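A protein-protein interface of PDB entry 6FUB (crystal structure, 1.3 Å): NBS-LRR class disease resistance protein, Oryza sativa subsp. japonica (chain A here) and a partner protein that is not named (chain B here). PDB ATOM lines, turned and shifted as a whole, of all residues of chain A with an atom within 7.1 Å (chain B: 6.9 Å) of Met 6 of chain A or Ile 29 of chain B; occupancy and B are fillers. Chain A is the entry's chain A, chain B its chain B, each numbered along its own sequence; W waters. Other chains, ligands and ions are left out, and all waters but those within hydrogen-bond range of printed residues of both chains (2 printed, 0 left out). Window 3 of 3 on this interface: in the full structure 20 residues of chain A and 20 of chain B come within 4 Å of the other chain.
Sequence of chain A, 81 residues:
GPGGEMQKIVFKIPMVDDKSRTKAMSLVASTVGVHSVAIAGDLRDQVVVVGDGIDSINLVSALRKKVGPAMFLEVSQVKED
OG of Ser 36 of chain A sits at hydrogen-bond distance from ND2 of Asn 26 of chain B (2.5 Å).
OD1 of Asn 26 of chain B is in hydrogen-bond range of N of Gly 28 of chain B (3.0 Å). The backbone carbonyl oxygen (O) of Pro 30 of chain B sits at hydrogen-bond distance from the side-chain hydroxyl (OH) of Tyr 51 of chain B (2.6 Å). The backbone NH (N) of Met 6 of chain A is in hydrogen-bond range of the side-chain carboxylate (OE2) of Glu 80 of chain A, at 2.8 Å. A ring nitrogen (ND1) of His 35 of chain A lies within hydrogen-bond range of the side-chain hydroxyl (OG) of Ser 36 of chain A, at 3.0 Å. The backbone NH (N) of His 35 of chain A lies within hydrogen-bond range of the backbone carbonyl oxygen (O) of Val 50 of chain A. The backbone carbonyl oxygen (O) of Ser 36 of chain A sits at hydrogen-bond distance from the backbone NH (N) of Val 50 of chain A.
Ile 29 of chain B touches Met 6 of chain A. Val 50 of chain A touches Asn 26 of chain B. Val 50 of chain A touches Ile 29 of chain B (CG1 to CD1, 3.97 Å). CB of Ile 29 of chain B touches CG1 of Val 78 of chain A, 3.9 Å away. Pro 30 of chain B touches Val 78 of chain A. CG1 of Val 78 of chain A touches OH of Tyr 51 of chain B, 3.6 Å away. Lys 79 of chain A touches Pro 30 of chain B (O to CG, 3.4 Å). CB of Lys 79 of chain A touches CG of Tyr 51 of chain B, 3.6 Å away.
Of the printed residues of chain B, Met 6 of chain A touches Ile 29. Gly 28 of chain B touches none of the printed residues of chain A. Printed residues of chain A within 4 Å of Asn 26 of chain B: Ser 36 and Val 50. Of the printed residues of chain B, Ser 36 of chain A touches Asn 26 (2.5 Å). Printed residues of chain A within 4 Å of Tyr 51 of chain B: Val 78 (3.6 Å) and Lys 79 (3.6 Å). Of the printed residues of chain A, Pro 30 of chain B touches Val 78 (3.9 Å) and Lys 79 (3.4 Å). Of the printed residues of chain B, Val 50 of chain A touches Asn 26 (3.5 Å) and Ile 29 (3.97 Å). The nearest residue of chain B that does not touch Met 6 of chain A is Gly 28 of chain B (5.2 Å). The nearest printed residue of chain A that does not touch Asn 26 of chain B is His 35 of chain A (4.6 Å).
Printed residues of chain B that touch a printed residue of chain A: Asn 26, Ile 29, Pro 30 and Tyr 51. Hydrophobic or aromatic side chains of chain B within 4 Å of the printed part of chain A: Ile 29, Pro 30 and Tyr 51. Printed residues of chain A that touch a printed residue of chain B: Met 6, Ser 36, Val 50, Val 78 and Lys 79. Hydrophobic or aromatic side chains of chain A that line the printed part of chain B: Met 6, Val 50 and Val 78. Among the printed residues, 9 pairs touch across the chains. Among the printed residues, no Asp or Glu carboxylate lies within 4 Å of a Lys or Arg side-chain nitrogen of the other chain.
Water W2 bridges NZ of Lys 8 of chain A (2.9 Å) and OH of Tyr 51 of chain B (3.0 Å). Water W1 lies within hydrogen-bond range of ND2 of Asn 26 of chain B (3.0 Å) and O of Val 48 of chain A (3.1 Å).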
ATOM      1  N   GLY A   1     -35.116  -7.894  16.038  1.00  0.00           N
ATOM      2  CA  GLY A   1     -35.093  -6.446  15.683  1.00  0.00           C
ATOM      3  C   GLY A   1     -35.684  -5.593  16.780  1.00  0.00           C
ATOM      4  O   GLY A   1     -36.128  -6.139  17.807  1.00  0.00           O
ATOM      5  N   GLY A   4     -38.690  -6.679  19.041  1.00  0.00           N
ATOM      6  CA  GLY A   4     -38.809  -8.141  19.050  1.00  0.00           C
ATOM      7  C   GLY A   4     -37.584  -8.856  19.619  1.00  0.00           C
ATOM      8  O   GLY A   4     -37.294  -9.967  19.222  1.00  0.00           O
ATOM      9  N   GLU A   5     -36.881  -8.243  20.570  1.00  0.00           N
ATOM     10  CA  GLU A   5     -35.556  -8.752  20.980  1.00  0.00           C
ATOM     11  C   GLU A   5     -35.643 -10.026  21.816  1.00  0.00           C
ATOM     12  O   GLU A   5     -36.637 -10.251  22.477  1.00  0.00           O
ATOM     13  CB  GLU A   5     -34.794  -7.671  21.758  1.00  0.00           C
ATOM     14  CG  GLU A   5     -34.509  -6.400  20.942  1.00  0.00           C
ATOM     15  CD  GLU A   5     -35.520  -5.278  21.145  1.00  0.00           C
ATOM     16  OE1 GLU A   5     -35.172  -4.100  20.844  1.00  0.00           O
ATOM     17  OE2 GLU A   5     -36.654  -5.576  21.540  1.00  0.00           O
ATOM     18  N   MET A   6     -34.585 -10.846  21.760  1.00  0.00           N
ATOM     19  CA  MET A   6     -34.392 -11.895  22.717  1.00  0.00           C
ATOM     20  C   MET A   6     -34.236 -11.322  24.152  1.00  0.00           C
ATOM     21  O   MET A   6     -33.791 -10.181  24.386  1.00  0.00           O
ATOM     22  CB  MET A   6     -33.181 -12.764  22.372  1.00  0.00           C
ATOM     23  CG  MET A   6     -33.337 -13.425  21.005  1.00  0.00           C
ATOM     24  SD  MET A   6     -31.954 -14.481  20.582  1.00  0.00           S
ATOM     25  CE  MET A   6     -32.650 -15.879  21.389  1.00  0.00           C
ATOM     26  N   GLN A   7     -34.663 -12.151  25.096  1.00  0.00           N
ATOM     27  CA  GLN A   7     -34.418 -11.980  26.517  1.00  0.00           C
ATOM     28  C   GLN A   7     -32.974 -12.347  26.836  1.00  0.00           C
ATOM     29  O   GLN A   7     -32.458 -13.329  26.306  1.00  0.00           O
ATOM     30  CB  GLN A   7     -35.258 -12.976  27.310  1.00  0.00           C
ATOM     31  CG  GLN A   7     -36.757 -12.873  27.182  1.00  0.00           C
ATOM     32  CD  GLN A   7     -37.417 -14.113  27.747  1.00  0.00           C
ATOM     33  OE1 GLN A   7     -37.378 -15.172  27.141  1.00  0.00           O
ATOM     34  NE2 GLN A   7     -37.931 -14.020  28.929  1.00  0.00           N
ATOM     35  N   LYS A   8     -32.405 -11.622  27.796  1.00  0.00           N
ATOM     36  CA  LYS A   8     -31.149 -12.005  28.435  1.00  0.00           C
ATOM     37  C   LYS A   8     -31.408 -12.056  29.951  1.00  0.00           C
ATOM     38  O   LYS A   8     -31.863 -11.073  30.581  1.00  0.00           O
ATOM     39  CB  LYS A   8     -30.064 -11.006  28.138  1.00  0.00           C
ATOM     40  CG  LYS A   8     -28.704 -11.391  28.679  1.00  0.00           C
ATOM     41  CD  LYS A   8     -27.649 -10.322  28.314  1.00  0.00           C
ATOM     42  CE  LYS A   8     -26.270 -10.643  28.867  1.00  0.00           C
ATOM     43  NZ  LYS A   8     -25.235  -9.701  28.299  1.00  0.00           N
ATOM     44  N   GLY A  33     -38.007 -22.190  25.573  1.00  0.00           N
ATOM     45  CA  GLY A  33     -37.681 -20.807  25.213  1.00  0.00           C
ATOM     46  C   GLY A  33     -36.198 -20.501  25.132  1.00  0.00           C
ATOM     47  O   GLY A  33     -35.794 -19.502  24.524  1.00  0.00           O
ATOM     48  N   VAL A  34     -35.377 -21.348  25.727  1.00  0.00           N
ATOM     49  CA  VAL A  34     -33.934 -21.107  25.787  1.00  0.00           C
ATOM     50  C   VAL A  34     -33.334 -21.337  24.402  1.00  0.00           C
ATOM     51  O   VAL A  34     -33.566 -22.368  23.767  1.00  0.00           O
ATOM     52  CB  VAL A  34     -33.233 -21.980  26.869  1.00  0.00           C
ATOM     53  CG1 VAL A  34     -31.704 -21.931  26.762  1.00  0.00           C
ATOM     54  CG2 VAL A  34     -33.659 -21.539  28.237  1.00  0.00           C
ATOM     55  N   HIS A  35     -32.557 -20.354  23.967  1.00  0.00           N
ATOM     56  CA  HIS A  35     -31.732 -20.438  22.775  1.00  0.00           C
ATOM     57  C   HIS A  35     -30.341 -20.970  23.104  1.00  0.00           C
ATOM     58  O   HIS A  35     -29.795 -21.832  22.384  1.00  0.00           O
ATOM     59  CB  HIS A  35     -31.637 -19.042  22.132  1.00  0.00           C
ATOM     60  CG  HIS A  35     -30.716 -18.967  20.966  1.00  0.00           C
ATOM     61  ND1 HIS A  35     -29.361 -18.738  21.104  1.00  0.00           N
ATOM     62  CD2 HIS A  35     -30.958 -19.047  19.635  1.00  0.00           C
ATOM     63  CE1 HIS A  35     -28.805 -18.722  19.901  1.00  0.00           C
ATOM     64  NE2 HIS A  35     -29.752 -18.901  18.998  1.00  0.00           N
ATOM     65  N   SER A  36     -29.742 -20.431  24.158  1.00  0.00           N
ATOM     66  CA  SER A  36     -28.388 -20.817  24.518  1.00  0.00           C
ATOM     67  C   SER A  36     -28.039 -20.384  25.914  1.00  0.00           C
ATOM     68  O   SER A  36     -28.763 -19.540  26.489  1.00  0.00           O
ATOM     69  CB  SER A  36     -27.383 -20.279  23.508  1.00  0.00           C
ATOM     70  OG  SER A  36     -27.437 -18.889  23.373  1.00  0.00           O
ATOM     71  N   VAL A  48     -25.445 -17.171  32.027  1.00  0.00           N
ATOM     72  CA  VAL A  48     -26.055 -16.210  31.099  1.00  0.00           C
ATOM     73  C   VAL A  48     -26.967 -16.978  30.159  1.00  0.00           C
ATOM     74  O   VAL A  48     -26.475 -17.768  29.326  1.00  0.00           O
ATOM     75  CB  VAL A  48     -24.950 -15.464  30.294  1.00  0.00           C
ATOM     76  CG1 VAL A  48     -25.557 -14.467  29.330  1.00  0.00           C
ATOM     77  CG2 VAL A  48     -23.940 -14.815  31.231  1.00  0.00           C
ATOM     78  N   VAL A  50     -29.935 -16.804  27.139  1.00  0.00           N
ATOM     79  CA  VAL A  50     -30.652 -16.006  26.142  1.00  0.00           C
ATOM     80  C   VAL A  50     -31.731 -16.840  25.470  1.00  0.00           C
ATOM     81  O   VAL A  50     -31.616 -18.062  25.377  1.00  0.00           O
ATOM     82  CB  VAL A  50     -29.736 -15.319  25.130  1.00  0.00           C
ATOM     83  CG1 VAL A  50     -28.807 -14.356  25.845  1.00  0.00           C
ATOM     84  CG2 VAL A  50     -28.921 -16.302  24.341  1.00  0.00           C
ATOM     85  N   GLY A  51     -32.843 -16.184  25.128  1.00  0.00           N
ATOM     86  CA  GLY A  51     -33.936 -16.892  24.492  1.00  0.00           C
ATOM     87  C   GLY A  51     -35.155 -16.016  24.319  1.00  0.00           C
ATOM     88  O   GLY A  51     -35.060 -14.791  24.304  1.00  0.00           O
ATOM     89  N   ASP A  52     -36.302 -16.667  24.164  1.00  0.00           N
ATOM     90  CA  ASP A  52     -37.535 -15.997  23.840  1.00  0.00           C
ATOM     91  C   ASP A  52     -38.624 -16.693  24.604  1.00  0.00           C
ATOM     92  O   ASP A  52     -38.735 -17.906  24.545  1.00  0.00           O
ATOM     93  CB  ASP A  52     -37.870 -16.079  22.343  1.00  0.00           C
ATOM     94  CG  ASP A  52     -36.893 -15.317  21.450  1.00  0.00           C
ATOM     95  OD1 ASP A  52     -37.083 -14.095  21.293  1.00  0.00           O
ATOM     96  OD2 ASP A  52     -35.962 -15.944  20.873  1.00  0.00           O
ATOM     97  N   GLY A  53     -39.440 -15.932  25.310  1.00  0.00           N
ATOM     98  CA  GLY A  53     -40.574 -16.528  26.030  1.00  0.00           C
ATOM     99  C   GLY A  53     -40.208 -17.460  27.176  1.00  0.00           C
ATOM    100  O   GLY A  53     -40.985 -18.334  27.555  1.00  0.00           O
ATOM    101  N   SER A  76     -32.561  -8.328  31.045  1.00  0.00           N
ATOM    102  CA  SER A  76     -32.493  -7.305  30.040  1.00  0.00           C
ATOM    103  C   SER A  76     -32.913  -7.859  28.705  1.00  0.00           C
ATOM    104  O   SER A  76     -33.201  -9.030  28.571  1.00  0.00           O
ATOM    105  CB  SER A  76     -31.090  -6.737  30.004  1.00  0.00           C
ATOM    106  OG  SER A  76     -30.108  -7.716  29.623  1.00  0.00           O
ATOM    107  N   GLN A  77     -32.961  -6.962  27.722  1.00  0.00           N
ATOM    108  CA  GLN A  77     -33.188  -7.308  26.330  1.00  0.00           C
ATOM    109  C   GLN A  77     -31.896  -7.256  25.534  1.00  0.00           C
ATOM    110  O   GLN A  77     -31.044  -6.378  25.787  1.00  0.00           O
ATOM    111  CB  GLN A  77     -34.242  -6.386  25.702  1.00  0.00           C
ATOM    112  CG  GLN A  77     -35.605  -6.476  26.346  1.00  0.00           C
ATOM    113  CD  GLN A  77     -36.300  -7.770  25.979  1.00  0.00           C
ATOM    114  OE1 GLN A  77     -36.473  -8.657  26.823  1.00  0.00           O
ATOM    115  NE2 GLN A  77     -36.686  -7.902  24.692  1.00  0.00           N
ATOM    116  N   VAL A  78     -31.739  -8.196  24.608  1.00  0.00           N
ATOM    117  CA  VAL A  78     -30.595  -8.155  23.702  1.00  0.00           C
ATOM    118  C   VAL A  78     -30.722  -6.973  22.747  1.00  0.00           C
ATOM    119  O   VAL A  78     -31.810  -6.720  22.267  1.00  0.00           O
ATOM    120  CB  VAL A  78     -30.481  -9.490  22.947  1.00  0.00           C
ATOM    121  CG1 VAL A  78     -29.370  -9.447  21.880  1.00  0.00           C
ATOM    122  CG2 VAL A  78     -30.239 -10.631  23.913  1.00  0.00           C
ATOM    123  N   LYS A  79     -29.679  -6.170  22.599  1.00  0.00           N
ATOM    124  CA  LYS A  79     -29.659  -5.089  21.660  1.00  0.00           C
ATOM    125  C   LYS A  79     -29.437  -5.584  20.249  1.00  0.00           C
ATOM    126  O   LYS A  79     -28.383  -6.145  19.952  1.00  0.00           O
ATOM    127  CB  LYS A  79     -28.631  -4.065  22.051  1.00  0.00           C
ATOM    128  CG  LYS A  79     -28.629  -2.844  21.193  1.00  0.00           C
ATOM    129  CD  LYS A  79     -27.663  -1.760  21.538  1.00  0.00           C
ATOM    130  CE  LYS A  79     -26.249  -1.987  21.168  1.00  0.00           C
ATOM    131  NZ  LYS A  79     -25.390  -0.736  21.331  1.00  0.00           N
ATOM    132  N   GLU A  80     -30.427  -5.431  19.371  1.00  0.00           N
ATOM    133  CA  GLU A  80     -30.391  -6.082  18.017  1.00  0.00           C
ATOM    134  C   GLU A  80     -30.931  -5.102  17.035  1.00  0.00           C
ATOM    135  O   GLU A  80     -32.083  -4.725  17.156  1.00  0.00           O
ATOM    136  CB  GLU A  80     -31.386  -7.257  17.962  1.00  0.00           C
ATOM    137  CG  GLU A  80     -31.203  -8.361  18.968  1.00  0.00           C
ATOM    138  CD  GLU A  80     -32.320  -9.386  18.936  1.00  0.00           C
ATOM    139  OE1 GLU A  80     -32.966  -9.484  17.867  1.00  0.00           O
ATOM    140  OE2 GLU A  80     -32.538 -10.089  19.981  1.00  0.00           O
ATOM    141  N   ASP B  25     -18.698 -14.422  24.562  1.00  0.00           N
ATOM    142  CA  ASP B  25     -19.473 -13.744  23.536  1.00  0.00           C
ATOM    143  C   ASP B  25     -20.297 -14.788  22.833  1.00  0.00           C
ATOM    144  O   ASP B  25     -19.827 -15.469  21.972  1.00  0.00           O
ATOM    145  CB  ASP B  25     -18.579 -13.005  22.543  1.00  0.00           C
ATOM    146  CG  ASP B  25     -17.971 -11.767  23.111  1.00  0.00           C
ATOM    147  OD1 ASP B  25     -18.567 -11.094  23.967  1.00  0.00           O
ATOM    148  OD2 ASP B  25     -16.878 -11.393  22.710  1.00  0.00           O
ATOM    149  N   ASN B  26     -21.555 -14.875  23.178  1.00  0.00           N
ATOM    150  CA  ASN B  26     -22.437 -15.902  22.658  1.00  0.00           C
ATOM    151  C   ASN B  26     -22.572 -15.661  21.162  1.00  0.00           C
ATOM    152  O   ASN B  26     -23.025 -14.576  20.776  1.00  0.00           O
ATOM    153  CB  ASN B  26     -23.790 -15.740  23.356  1.00  0.00           C
ATOM    154  CG  ASN B  26     -24.810 -16.794  22.974  1.00  0.00           C
ATOM    155  OD1 ASN B  26     -24.968 -17.144  21.790  1.00  0.00           O
ATOM    156  ND2 ASN B  26     -25.561 -17.275  23.979  1.00  0.00           N
ATOM    157  N   PRO B  27     -22.180 -16.637  20.334  1.00  0.00           N
ATOM    158  CA  PRO B  27     -22.153 -16.416  18.869  1.00  0.00           C
ATOM    159  C   PRO B  27     -23.524 -16.167  18.225  1.00  0.00           C
ATOM    160  O   PRO B  27     -23.581 -15.707  17.076  1.00  0.00           O
ATOM    161  CB  PRO B  27     -21.515 -17.711  18.336  1.00  0.00           C
ATOM    162  CG  PRO B  27     -21.803 -18.759  19.380  1.00  0.00           C
ATOM    163  CD  PRO B  27     -21.753 -18.010  20.694  1.00  0.00           C
ATOM    164  N   GLY B  28     -24.611 -16.514  18.902  1.00  0.00           N
ATOM    165  CA  GLY B  28     -25.956 -16.267  18.376  1.00  0.00           C
ATOM    166  C   GLY B  28     -26.520 -14.855  18.419  1.00  0.00           C
ATOM    167  O   GLY B  28     -27.563 -14.593  17.792  1.00  0.00           O
ATOM    168  N   ILE B  29     -25.886 -13.954  19.181  1.00  0.00           N
ATOM    169  CA  ILE B  29     -26.438 -12.601  19.438  1.00  0.00           C
ATOM    170  C   ILE B  29     -25.339 -11.571  19.202  1.00  0.00           C
ATOM    171  O   ILE B  29     -24.176 -11.906  19.225  1.00  0.00           O
ATOM    172  CB  ILE B  29     -26.983 -12.425  20.866  1.00  0.00           C
ATOM    173  CG1 ILE B  29     -25.898 -12.632  21.936  1.00  0.00           C
ATOM    174  CG2 ILE B  29     -28.175 -13.350  21.072  1.00  0.00           C
ATOM    175  CD1 ILE B  29     -26.359 -12.444  23.379  1.00  0.00           C
ATOM    176  N   PRO B  30     -25.712 -10.315  18.972  1.00  0.00           N
ATOM    177  CA  PRO B  30     -24.688  -9.270  18.802  1.00  0.00           C
ATOM    178  C   PRO B  30     -23.707  -9.172  19.944  1.00  0.00           C
ATOM    179  O   PRO B  30     -24.087  -9.462  21.089  1.00  0.00           O
ATOM    180  CB  PRO B  30     -25.516  -7.995  18.631  1.00  0.00           C
ATOM    181  CG  PRO B  30     -26.799  -8.482  18.071  1.00  0.00           C
ATOM    182  CD  PRO B  30     -27.079  -9.796  18.750  1.00  0.00           C
ATOM    183  N   VAL B  31     -22.452  -8.865  19.627  1.00  0.00           N
ATOM    184  CA  VAL B  31     -21.411  -8.812  20.634  1.00  0.00           C
ATOM    185  C   VAL B  31     -21.645  -7.521  21.471  1.00  0.00           C
ATOM    186  O   VAL B  31     -21.636  -6.409  20.926  1.00  0.00           O
ATOM    187  CB  VAL B  31     -20.018  -8.849  19.982  1.00  0.00           C
ATOM    188  CG1 VAL B  31     -18.935  -8.679  21.027  1.00  0.00           C
ATOM    189  CG2 VAL B  31     -19.864 -10.156  19.168  1.00  0.00           C
ATOM    190  N   PRO B  32     -21.732  -7.640  22.792  1.00  0.00           N
ATOM    191  CA  PRO B  32     -21.860  -6.459  23.605  1.00  0.00           C
ATOM    192  C   PRO B  32     -20.602  -5.615  23.649  1.00  0.00           C
ATOM    193  O   PRO B  32     -19.480  -6.148  23.662  1.00  0.00           O
ATOM    194  CB  PRO B  32     -22.303  -7.015  24.968  1.00  0.00           C
ATOM    195  CG  PRO B  32     -21.626  -8.351  24.974  1.00  0.00           C
ATOM    196  CD  PRO B  32     -21.779  -8.866  23.577  1.00  0.00           C
ATOM    197  N   TYR B  51     -24.428  -4.136  26.705  1.00  0.00           N
ATOM    198  CA  TYR B  51     -24.538  -3.321  25.562  1.00  0.00           C
ATOM    199  C   TYR B  51     -24.362  -1.846  25.826  1.00  0.00           C
ATOM    200  O   TYR B  51     -24.800  -1.368  26.909  1.00  0.00           O
ATOM    201  CB  TYR B  51     -25.827  -3.596  24.773  1.00  0.00           C
ATOM    202  CG  TYR B  51     -25.920  -4.966  24.241  1.00  0.00           C
ATOM    203  CD1 TYR B  51     -25.199  -5.313  23.098  1.00  0.00           C
ATOM    204  CD2 TYR B  51     -26.650  -5.936  24.846  1.00  0.00           C
ATOM    205  CE1 TYR B  51     -25.232  -6.628  22.623  1.00  0.00           C
ATOM    206  CE2 TYR B  51     -26.670  -7.240  24.420  1.00  0.00           C
ATOM    207  CZ  TYR B  51     -25.958  -7.622  23.279  1.00  0.00           C
ATOM    208  OH  TYR B  51     -25.958  -8.935  22.850  1.00  0.00           O
HETATM  209  O   HOH W   1     -24.890 -16.870  26.827  1.00  0.00           O
HETATM  210  O   HOH W   2     -24.924 -10.012  25.481  1.00  0.00           O
